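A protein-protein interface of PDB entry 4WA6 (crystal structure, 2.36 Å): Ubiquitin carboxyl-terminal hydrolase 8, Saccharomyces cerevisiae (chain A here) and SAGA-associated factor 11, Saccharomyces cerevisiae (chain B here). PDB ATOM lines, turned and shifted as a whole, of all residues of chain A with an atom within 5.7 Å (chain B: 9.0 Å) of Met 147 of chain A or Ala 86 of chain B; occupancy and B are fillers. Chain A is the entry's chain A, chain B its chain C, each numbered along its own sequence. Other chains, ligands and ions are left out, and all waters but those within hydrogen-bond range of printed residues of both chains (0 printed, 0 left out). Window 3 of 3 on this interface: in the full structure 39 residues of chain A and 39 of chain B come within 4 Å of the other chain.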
ATOM      1  N   ILE A 145     -33.275  18.637  22.837  1.00  0.00           N
ATOM      2  CA  ILE A 145     -33.629  20.032  22.994  1.00  0.00           C
ATOM      3  C   ILE A 145     -32.370  20.860  22.857  1.00  0.00           C
ATOM      4  O   ILE A 145     -31.299  20.438  23.278  1.00  0.00           O
ATOM      5  CB  ILE A 145     -34.342  20.271  24.338  1.00  0.00           C
ATOM      6  CG1 ILE A 145     -35.629  19.448  24.365  1.00  0.00           C
ATOM      7  CG2 ILE A 145     -34.672  21.753  24.555  1.00  0.00           C
ATOM      8  CD1 ILE A 145     -36.133  19.141  25.760  1.00  0.00           C
ATOM      9  N   ASN A 146     -32.494  22.013  22.207  1.00  0.00           N
ATOM     10  CA  ASN A 146     -31.365  22.898  22.052  1.00  0.00           C
ATOM     11  C   ASN A 146     -31.127  23.510  23.406  1.00  0.00           C
ATOM     12  O   ASN A 146     -32.054  23.993  24.059  1.00  0.00           O
ATOM     13  CB  ASN A 146     -31.589  23.969  20.972  1.00  0.00           C
ATOM     14  CG  ASN A 146     -30.313  24.754  20.653  1.00  0.00           C
ATOM     15  OD1 ASN A 146     -29.433  24.876  21.499  1.00  0.00           O
ATOM     16  ND2 ASN A 146     -30.203  25.277  19.430  1.00  0.00           N
ATOM     17  N   MET A 147     -29.877  23.471  23.835  1.00  0.00           N
ATOM     18  CA  MET A 147     -29.555  23.821  25.184  1.00  0.00           C
ATOM     19  C   MET A 147     -28.634  25.030  25.277  1.00  0.00           C
ATOM     20  O   MET A 147     -27.992  25.257  26.313  1.00  0.00           O
ATOM     21  CB  MET A 147     -28.998  22.587  25.857  1.00  0.00           C
ATOM     22  CG  MET A 147     -30.137  21.636  26.132  1.00  0.00           C
ATOM     23  SD  MET A 147     -29.708  20.077  26.892  1.00  0.00           S
ATOM     24  CE  MET A 147     -31.355  19.385  26.982  1.00  0.00           C
ATOM     25  N   GLY A 148     -28.654  25.849  24.223  1.00  0.00           N
ATOM     26  CA  GLY A 148     -27.762  26.998  24.093  1.00  0.00           C
ATOM     27  C   GLY A 148     -26.864  26.788  22.892  1.00  0.00           C
ATOM     28  O   GLY A 148     -25.686  26.510  23.020  1.00  0.00           O
ATOM     29  N   SER A 149     -27.442  26.891  21.710  1.00  0.00           N
ATOM     30  CA  SER A 149     -26.688  26.726  20.502  1.00  0.00           C
ATOM     31  C   SER A 149     -26.034  25.341  20.448  1.00  0.00           C
ATOM     32  O   SER A 149     -24.793  25.205  20.394  1.00  0.00           O
ATOM     33  CB  SER A 149     -25.657  27.852  20.382  1.00  0.00           C
ATOM     34  OG  SER A 149     -26.184  28.900  19.595  1.00  0.00           O
ATOM     35  N   THR A 150     -26.861  24.301  20.425  1.00  0.00           N
ATOM     36  CA  THR A 150     -26.308  22.949  20.398  1.00  0.00           C
ATOM     37  C   THR A 150     -26.824  22.047  19.280  1.00  0.00           C
ATOM     38  O   THR A 150     -26.664  20.829  19.345  1.00  0.00           O
ATOM     39  CB  THR A 150     -26.514  22.234  21.763  1.00  0.00           C
ATOM     40  OG1 THR A 150     -27.915  22.212  22.104  1.00  0.00           O
ATOM     41  CG2 THR A 150     -25.694  22.907  22.821  1.00  0.00           C
ATOM     42  N   GLN A 218     -33.206  13.243  27.570  1.00  0.00           N
ATOM     43  CA  GLN A 218     -32.150  14.210  27.385  1.00  0.00           C
ATOM     44  C   GLN A 218     -30.931  13.978  28.261  1.00  0.00           C
ATOM     45  O   GLN A 218     -29.988  14.774  28.195  1.00  0.00           O
ATOM     46  CB  GLN A 218     -32.688  15.594  27.740  1.00  0.00           C
ATOM     47  CG  GLN A 218     -33.964  15.966  26.986  1.00  0.00           C
ATOM     48  CD  GLN A 218     -33.746  16.072  25.481  1.00  0.00           C
ATOM     49  OE1 GLN A 218     -32.677  16.456  25.041  1.00  0.00           O
ATOM     50  NE2 GLN A 218     -34.765  15.749  24.696  1.00  0.00           N
ATOM     51  N   PHE A 221     -27.496  13.116  26.479  1.00  0.00           N
ATOM     52  CA  PHE A 221     -27.086  14.411  25.882  1.00  0.00           C
ATOM     53  C   PHE A 221     -26.499  15.402  26.864  1.00  0.00           C
ATOM     54  O   PHE A 221     -25.493  16.042  26.579  1.00  0.00           O
ATOM     55  CB  PHE A 221     -28.284  15.084  25.194  1.00  0.00           C
ATOM     56  CG  PHE A 221     -27.916  16.265  24.332  1.00  0.00           C
ATOM     57  CD1 PHE A 221     -26.749  16.279  23.587  1.00  0.00           C
ATOM     58  CD2 PHE A 221     -28.773  17.339  24.231  1.00  0.00           C
ATOM     59  CE1 PHE A 221     -26.419  17.358  22.811  1.00  0.00           C
ATOM     60  CE2 PHE A 221     -28.451  18.423  23.424  1.00  0.00           C
ATOM     61  CZ  PHE A 221     -27.267  18.438  22.723  1.00  0.00           C
ATOM     62  N   ILE A 222     -27.122  15.531  28.027  1.00  0.00           N
ATOM     63  CA  ILE A 222     -26.555  16.342  29.101  1.00  0.00           C
ATOM     64  C   ILE A 222     -25.212  15.806  29.541  1.00  0.00           C
ATOM     65  O   ILE A 222     -24.287  16.563  29.762  1.00  0.00           O
ATOM     66  CB  ILE A 222     -27.474  16.367  30.357  1.00  0.00           C
ATOM     67  CG1 ILE A 222     -28.720  17.214  30.076  1.00  0.00           C
ATOM     68  CG2 ILE A 222     -26.734  16.923  31.554  1.00  0.00           C
ATOM     69  CD1 ILE A 222     -29.952  16.732  30.805  1.00  0.00           C
ATOM     70  N   LEU A 225     -22.723  16.745  27.073  1.00  0.00           N
ATOM     71  CA  LEU A 225     -22.269  18.130  27.250  1.00  0.00           C
ATOM     72  C   LEU A 225     -21.363  18.251  28.455  1.00  0.00           C
ATOM     73  O   LEU A 225     -20.452  19.078  28.481  1.00  0.00           O
ATOM     74  CB  LEU A 225     -23.455  19.074  27.435  1.00  0.00           C
ATOM     75  CG  LEU A 225     -24.371  19.138  26.213  1.00  0.00           C
ATOM     76  CD1 LEU A 225     -25.720  19.731  26.573  1.00  0.00           C
ATOM     77  CD2 LEU A 225     -23.695  19.919  25.101  1.00  0.00           C
ATOM     78  N   GLU B  66     -39.377  27.028  23.861  1.00  0.00           N
ATOM     79  CA  GLU B  66     -38.269  26.697  24.742  1.00  0.00           C
ATOM     80  C   GLU B  66     -38.317  27.461  26.081  1.00  0.00           C
ATOM     81  O   GLU B  66     -37.575  27.128  27.010  1.00  0.00           O
ATOM     82  CB  GLU B  66     -36.917  26.840  24.011  1.00  0.00           C
ATOM     83  CG  GLU B  66     -36.760  25.913  22.795  1.00  0.00           C
ATOM     84  CD  GLU B  66     -35.335  25.372  22.611  1.00  0.00           C
ATOM     85  OE1 GLU B  66     -34.628  25.206  23.631  1.00  0.00           O
ATOM     86  OE2 GLU B  66     -34.915  25.092  21.454  1.00  0.00           O
ATOM     87  N   GLN B  69     -39.954  24.863  27.610  1.00  0.00           N
ATOM     88  CA  GLN B  69     -38.965  23.776  27.738  1.00  0.00           C
ATOM     89  C   GLN B  69     -38.199  23.894  29.053  1.00  0.00           C
ATOM     90  O   GLN B  69     -37.438  24.846  29.245  1.00  0.00           O
ATOM     91  CB  GLN B  69     -37.937  23.779  26.595  1.00  0.00           C
ATOM     92  CG  GLN B  69     -38.462  23.390  25.221  1.00  0.00           C
ATOM     93  CD  GLN B  69     -38.714  21.902  25.058  1.00  0.00           C
ATOM     94  OE1 GLN B  69     -38.602  21.125  26.009  1.00  0.00           O
ATOM     95  NE2 GLN B  69     -39.075  21.498  23.843  1.00  0.00           N
ATOM     96  N   TYR B  70     -38.371  22.912  29.933  1.00  0.00           N
ATOM     97  CA  TYR B  70     -37.723  22.939  31.237  1.00  0.00           C
ATOM     98  C   TYR B  70     -36.936  21.664  31.558  1.00  0.00           C
ATOM     99  O   TYR B  70     -37.433  20.563  31.335  1.00  0.00           O
ATOM    100  CB  TYR B  70     -38.774  23.151  32.327  1.00  0.00           C
ATOM    101  CG  TYR B  70     -39.241  24.585  32.486  1.00  0.00           C
ATOM    102  CD1 TYR B  70     -38.379  25.578  32.975  1.00  0.00           C
ATOM    103  CD2 TYR B  70     -40.560  24.952  32.186  1.00  0.00           C
ATOM    104  CE1 TYR B  70     -38.808  26.892  33.139  1.00  0.00           C
ATOM    105  CE2 TYR B  70     -40.999  26.261  32.352  1.00  0.00           C
ATOM    106  CZ  TYR B  70     -40.126  27.232  32.829  1.00  0.00           C
ATOM    107  OH  TYR B  70     -40.570  28.537  32.994  1.00  0.00           O
ATOM    108  N   ILE B  71     -35.700  21.834  32.052  1.00  0.00           N
ATOM    109  CA  ILE B  71     -35.012  20.839  32.915  1.00  0.00           C
ATOM    110  C   ILE B  71     -34.115  21.569  33.917  1.00  0.00           C
ATOM    111  O   ILE B  71     -33.557  20.971  34.839  1.00  0.00           O
ATOM    112  CB  ILE B  71     -34.117  19.835  32.159  1.00  0.00           C
ATOM    113  CG1 ILE B  71     -34.821  19.310  30.897  1.00  0.00           C
ATOM    114  CG2 ILE B  71     -33.701  18.705  33.110  1.00  0.00           C
ATOM    115  CD1 ILE B  71     -33.915  18.591  29.922  1.00  0.00           C
ATOM    116  N   VAL B  80     -34.490  24.246  35.060  1.00  0.00           N
ATOM    117  CA  VAL B  80     -33.712  25.065  34.127  1.00  0.00           C
ATOM    118  C   VAL B  80     -34.406  25.169  32.762  1.00  0.00           C
ATOM    119  O   VAL B  80     -34.666  24.151  32.108  1.00  0.00           O
ATOM    120  CB  VAL B  80     -32.283  24.526  33.942  1.00  0.00           C
ATOM    121  CG1 VAL B  80     -31.501  25.402  32.974  1.00  0.00           C
ATOM    122  CG2 VAL B  80     -31.584  24.441  35.289  1.00  0.00           C
ATOM    123  N   SER B  81     -34.728  26.406  32.359  1.00  0.00           N
ATOM    124  CA  SER B  81     -35.160  26.694  30.988  1.00  0.00           C
ATOM    125  C   SER B  81     -34.172  25.973  30.057  1.00  0.00           C
ATOM    126  O   SER B  81     -32.966  26.237  30.078  1.00  0.00           O
ATOM    127  CB  SER B  81     -35.192  28.212  30.714  1.00  0.00           C
ATOM    128  OG  SER B  81     -35.834  28.513  29.473  1.00  0.00           O
ATOM    129  N   ALA B  82     -34.684  25.015  29.300  1.00  0.00           N
ATOM    130  CA  ALA B  82     -33.829  24.137  28.499  1.00  0.00           C
ATOM    131  C   ALA B  82     -32.840  24.938  27.671  1.00  0.00           C
ATOM    132  O   ALA B  82     -31.652  24.705  27.769  1.00  0.00           O
ATOM    133  CB  ALA B  82     -34.678  23.249  27.609  1.00  0.00           C
ATOM    134  N   ASN B  83     -33.325  25.927  26.920  1.00  0.00           N
ATOM    135  CA  ASN B  83     -32.457  26.769  26.068  1.00  0.00           C
ATOM    136  C   ASN B  83     -31.316  27.515  26.762  1.00  0.00           C
ATOM    137  O   ASN B  83     -30.480  28.124  26.095  1.00  0.00           O
ATOM    138  CB  ASN B  83     -33.281  27.792  25.273  1.00  0.00           C
ATOM    139  CG  ASN B  83     -33.852  28.896  26.138  1.00  0.00           C
ATOM    140  OD1 ASN B  83     -33.144  29.816  26.559  1.00  0.00           O
ATOM    141  ND2 ASN B  83     -35.156  28.826  26.388  1.00  0.00           N
ATOM    142  N   ARG B  84     -31.303  27.506  28.091  1.00  0.00           N
ATOM    143  CA  ARG B  84     -30.254  28.142  28.868  1.00  0.00           C
ATOM    144  C   ARG B  84     -29.461  27.066  29.593  1.00  0.00           C
ATOM    145  O   ARG B  84     -28.572  27.363  30.369  1.00  0.00           O
ATOM    146  CB  ARG B  84     -30.883  29.131  29.860  1.00  0.00           C
ATOM    147  CG  ARG B  84     -30.963  30.578  29.379  1.00  0.00           C
ATOM    148  CD  ARG B  84     -29.840  31.425  29.984  1.00  0.00           C
ATOM    149  NE  ARG B  84     -30.083  32.871  29.882  1.00  0.00           N
ATOM    150  CZ  ARG B  84     -29.691  33.650  28.866  1.00  0.00           C
ATOM    151  NH1 ARG B  84     -29.029  33.141  27.830  1.00  0.00           N
ATOM    152  NH2 ARG B  84     -29.961  34.958  28.880  1.00  0.00           N
ATOM    153  N   LEU B  85     -29.754  25.804  29.298  1.00  0.00           N
ATOM    154  CA  LEU B  85     -29.223  24.699  30.093  1.00  0.00           C
ATOM    155  C   LEU B  85     -27.703  24.547  30.016  1.00  0.00           C
ATOM    156  O   LEU B  85     -27.090  24.179  30.998  1.00  0.00           O
ATOM    157  CB  LEU B  85     -29.925  23.384  29.722  1.00  0.00           C
ATOM    158  CG  LEU B  85     -29.642  22.167  30.611  1.00  0.00           C
ATOM    159  CD1 LEU B  85     -30.863  21.252  30.670  1.00  0.00           C
ATOM    160  CD2 LEU B  85     -28.414  21.397  30.140  1.00  0.00           C
ATOM    161  N   ALA B  86     -27.099  24.827  28.867  1.00  0.00           N
ATOM    162  CA  ALA B  86     -25.625  24.742  28.731  1.00  0.00           C
ATOM    163  C   ALA B  86     -24.954  25.885  29.465  1.00  0.00           C
ATOM    164  O   ALA B  86     -23.850  25.739  30.000  1.00  0.00           O
ATOM    165  CB  ALA B  86     -25.213  24.761  27.275  1.00  0.00           C
ATOM    166  N   ALA B  87     -25.631  27.031  29.468  1.00  0.00           N
ATOM    167  CA  ALA B  87     -25.251  28.165  30.313  1.00  0.00           C
ATOM    168  C   ALA B  87     -25.318  27.794  31.804  1.00  0.00           C
ATOM    169  O   ALA B  87     -24.368  28.033  32.554  1.00  0.00           O
ATOM    170  CB  ALA B  87     -26.128  29.387  30.011  1.00  0.00           C
ATOM    171  N   HIS B  88     -26.418  27.178  32.229  1.00  0.00           N
ATOM    172  CA  HIS B  88     -26.526  26.762  33.630  1.00  0.00           C
ATOM    173  C   HIS B  88     -25.428  25.749  34.003  1.00  0.00           C
ATOM    174  O   HIS B  88     -24.890  25.788  35.110  1.00  0.00           O
ATOM    175  CB  HIS B  88     -27.905  26.188  33.958  1.00  0.00           C
ATOM    176  CG  HIS B  88     -27.945  25.484  35.273  1.00  0.00           C
ATOM    177  ND1 HIS B  88     -27.720  26.138  36.463  1.00  0.00           N
ATOM    178  CD2 HIS B  88     -28.106  24.177  35.585  1.00  0.00           C
ATOM    179  CE1 HIS B  88     -27.787  25.270  37.460  1.00  0.00           C
ATOM    180  NE2 HIS B  88     -28.015  24.072  36.953  1.00  0.00           N
ATOM    181  N   LEU B  89     -25.108  24.861  33.070  1.00  0.00           N
ATOM    182  CA  LEU B  89     -24.037  23.876  33.255  1.00  0.00           C
ATOM    183  C   LEU B  89     -22.671  24.506  33.459  1.00  0.00           C
ATOM    184  O   LEU B  89     -21.937  24.090  34.344  1.00  0.00           O
ATOM    185  CB  LEU B  89     -23.973  22.920  32.068  1.00  0.00           C
ATOM    186  CG  LEU B  89     -24.960  21.768  32.180  1.00  0.00           C
ATOM    187  CD1 LEU B  89     -25.283  21.266  30.794  1.00  0.00           C
ATOM    188  CD2 LEU B  89     -24.383  20.646  33.020  1.00  0.00           C
ATOM    189  N   GLN B  90     -22.329  25.498  32.643  1.00  0.00           N
ATOM    190  CA  GLN B  90     -21.026  26.148  32.771  1.00  0.00           C
ATOM    191  C   GLN B  90     -20.765  26.480  34.235  1.00  0.00           C
ATOM    192  O   GLN B  90     -19.720  26.115  34.814  1.00  0.00           O
ATOM    193  CB  GLN B  90     -20.967  27.434  31.937  1.00  0.00           C
ATOM    194  CG  GLN B  90     -20.433  27.251  30.524  1.00  0.00           C
ATOM    195  CD  GLN B  90     -18.909  27.097  30.459  1.00  0.00           C
ATOM    196  OE1 GLN B  90     -18.285  26.491  31.336  1.00  0.00           O
ATOM    197  NE2 GLN B  90     -18.308  27.642  29.403  1.00  0.00           N
ATOM    198  N   ARG B  91     -21.757  27.154  34.811  1.00  0.00           N
ATOM    199  CA  ARG B  91     -21.714  27.625  36.180  1.00  0.00           C
ATOM    200  C   ARG B  91     -21.748  26.395  37.076  1.00  0.00           C
ATOM    201  O   ARG B  91     -20.766  26.055  37.739  1.00  0.00           O
ATOM    202  CB  ARG B  91     -22.930  28.566  36.452  1.00  0.00           C
ATOM    203  CG  ARG B  91     -22.761  29.642  37.531  1.00  0.00           C
ATOM    204  CD  ARG B  91     -24.078  30.372  37.841  1.00  0.00           C
ATOM    205  NE  ARG B  91     -24.608  31.232  36.759  1.00  0.00           N
ATOM    206  CZ  ARG B  91     -25.573  30.906  35.877  1.00  0.00           C
ATOM    207  NH1 ARG B  91     -26.185  29.720  35.890  1.00  0.00           N
ATOM    208  NH2 ARG B  91     -25.951  31.789  34.952  1.00  0.00           N
ATOM    209  N   CYS B  92     -22.877  25.695  37.025  1.00  0.00           N
ATOM    210  CA  CYS B  92     -23.251  24.742  38.068  1.00  0.00           C
ATOM    211  C   CYS B  92     -22.269  23.596  38.159  1.00  0.00           C
ATOM    212  O   CYS B  92     -22.054  23.084  39.243  1.00  0.00           O
ATOM    213  CB  CYS B  92     -24.707  24.256  37.891  1.00  0.00           C
ATOM    214  SG  CYS B  92     -25.038  22.569  38.388  1.00  0.00           S
ATOM    215  N   LEU B  93     -21.654  23.226  37.040  1.00  0.00           N
ATOM    216  CA  LEU B  93     -20.597  22.199  37.049  1.00  0.00           C
ATOM    217  C   LEU B  93     -19.247  22.649  37.619  1.00  0.00           C
ATOM    218  O   LEU B  93     -18.313  21.840  37.679  1.00  0.00           O
ATOM    219  CB  LEU B  93     -20.354  21.630  35.642  1.00  0.00           C
ATOM    220  CG  LEU B  93     -21.141  20.358  35.292  1.00  0.00           C
ATOM    221  CD1 LEU B  93     -21.177  20.131  33.778  1.00  0.00           C
ATOM    222  CD2 LEU B  93     -20.565  19.144  36.021  1.00  0.00           C
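Of the printed residues of chain B, Met 147 of chain A touches Ile 71, Ala 82, Asn 83, Leu 85 and Ala 86. Ala 86 of chain B touches just one residue of chain A: Met 147 (2.7 Å). Asn 146 of chain A touches just these residues of chain B: Glu 66 (2.9 Å), Ala 82 (3.8 Å) and Asn 83 (3.5 Å). Of the printed residues of chain B, Ile 145 of chain A touches Glu 66 (3.6 Å), Gln 69 (3.2 Å) and Ala 82 (3.4 Å). Of the printed residues of chain A, Ile 71 of chain B touches Met 147 and Gln 218. Cys 92 of chain B touches none of the printed residues of chain A. The nearest residue of chain B that does not touch Met 147 of chain A is Arg 84 of chain B (4.02 Å).
Of the 18 printed residues of chain B, 7 touch a printed residue of chain A. Hydrophobic or aromatic side chains of chain B that line the printed part of chain A: Ile 71, Ala 82, Leu 85 and Ala 86. Hydrophobic or aromatic side chains of chain A within 4 Å of the printed part of chain B: Ile 145 and Met 147. Among the printed residues, 13 pairs touch across the chains. Among the printed residues, no Asp or Glu carboxylate lies within 4 Å of a Lys or Arg side-chain nitrogen of the other chain.
The backbone NH of Ile 71 of chain B is in hydrogen-bond range of the backbone carbonyl oxygen of Val 80 of chain B (2.5 Å). The backbone NH (N) of Ile 145 of chain A is in hydrogen-bond range of the side-chain amide oxygen (OE1) of Gln 218 of chain A (3.2 Å). The backbone NH of Ser 149 of chain A sits at hydrogen-bond distance from the side-chain amide oxygen of Asn 146 of chain A, 2.8 Å away. OD1 of Asn 146 of chain A lies within hydrogen-bond range of N of Gly 148 of chain A (3.0 Å). The backbone carbonyl oxygen (O) of Gln 69 of chain B lies within hydrogen-bond range of the backbone NH (N) of Ala 82 of chain B (2.8 Å). N of Met 147 of chain A sits at hydrogen-bond distance from OG1 of Thr 150 of chain A (2.9 Å).
Among the printed residues, merely in contact across the chains: Ile 145 of chain A with Gln 69 of chain B (3.2 Å), Ile 145 of chain A with Ala 82 of chain B (3.4 Å), Met 147 of chain A with Ala 82 of chain B (3.4 Å), Asn 146 of chain A with Asn 83 of chain B (3.5 Å), Met 147 of chain A with Leu 85 of chain B (3.5 Å), Ile 145 of chain A with Glu 66 of chain B (3.6 Å), Met 147 of chain A with Asn 83 of chain B (3.7 Å), Asn 146 of chain A with Ala 82 of chain B (3.8 Å), Gln 218 of chain A with Ile 71 of chain B (3.9 Å) and Met 147 of chain A with Ile 71 of chain B (3.98 Å).
N of Ala 86 of chain B sits at hydrogen-bond distance from O of Met 147 of chain A, 2.7 Å away. OE1 of Glu 66 of chain B sits close to O of Asn 146 of chain A, 2.9 Å away. O of Asn 83 of chain B is in hydrogen-bond range of N of Gly 148 of chain A (3.5 Å).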
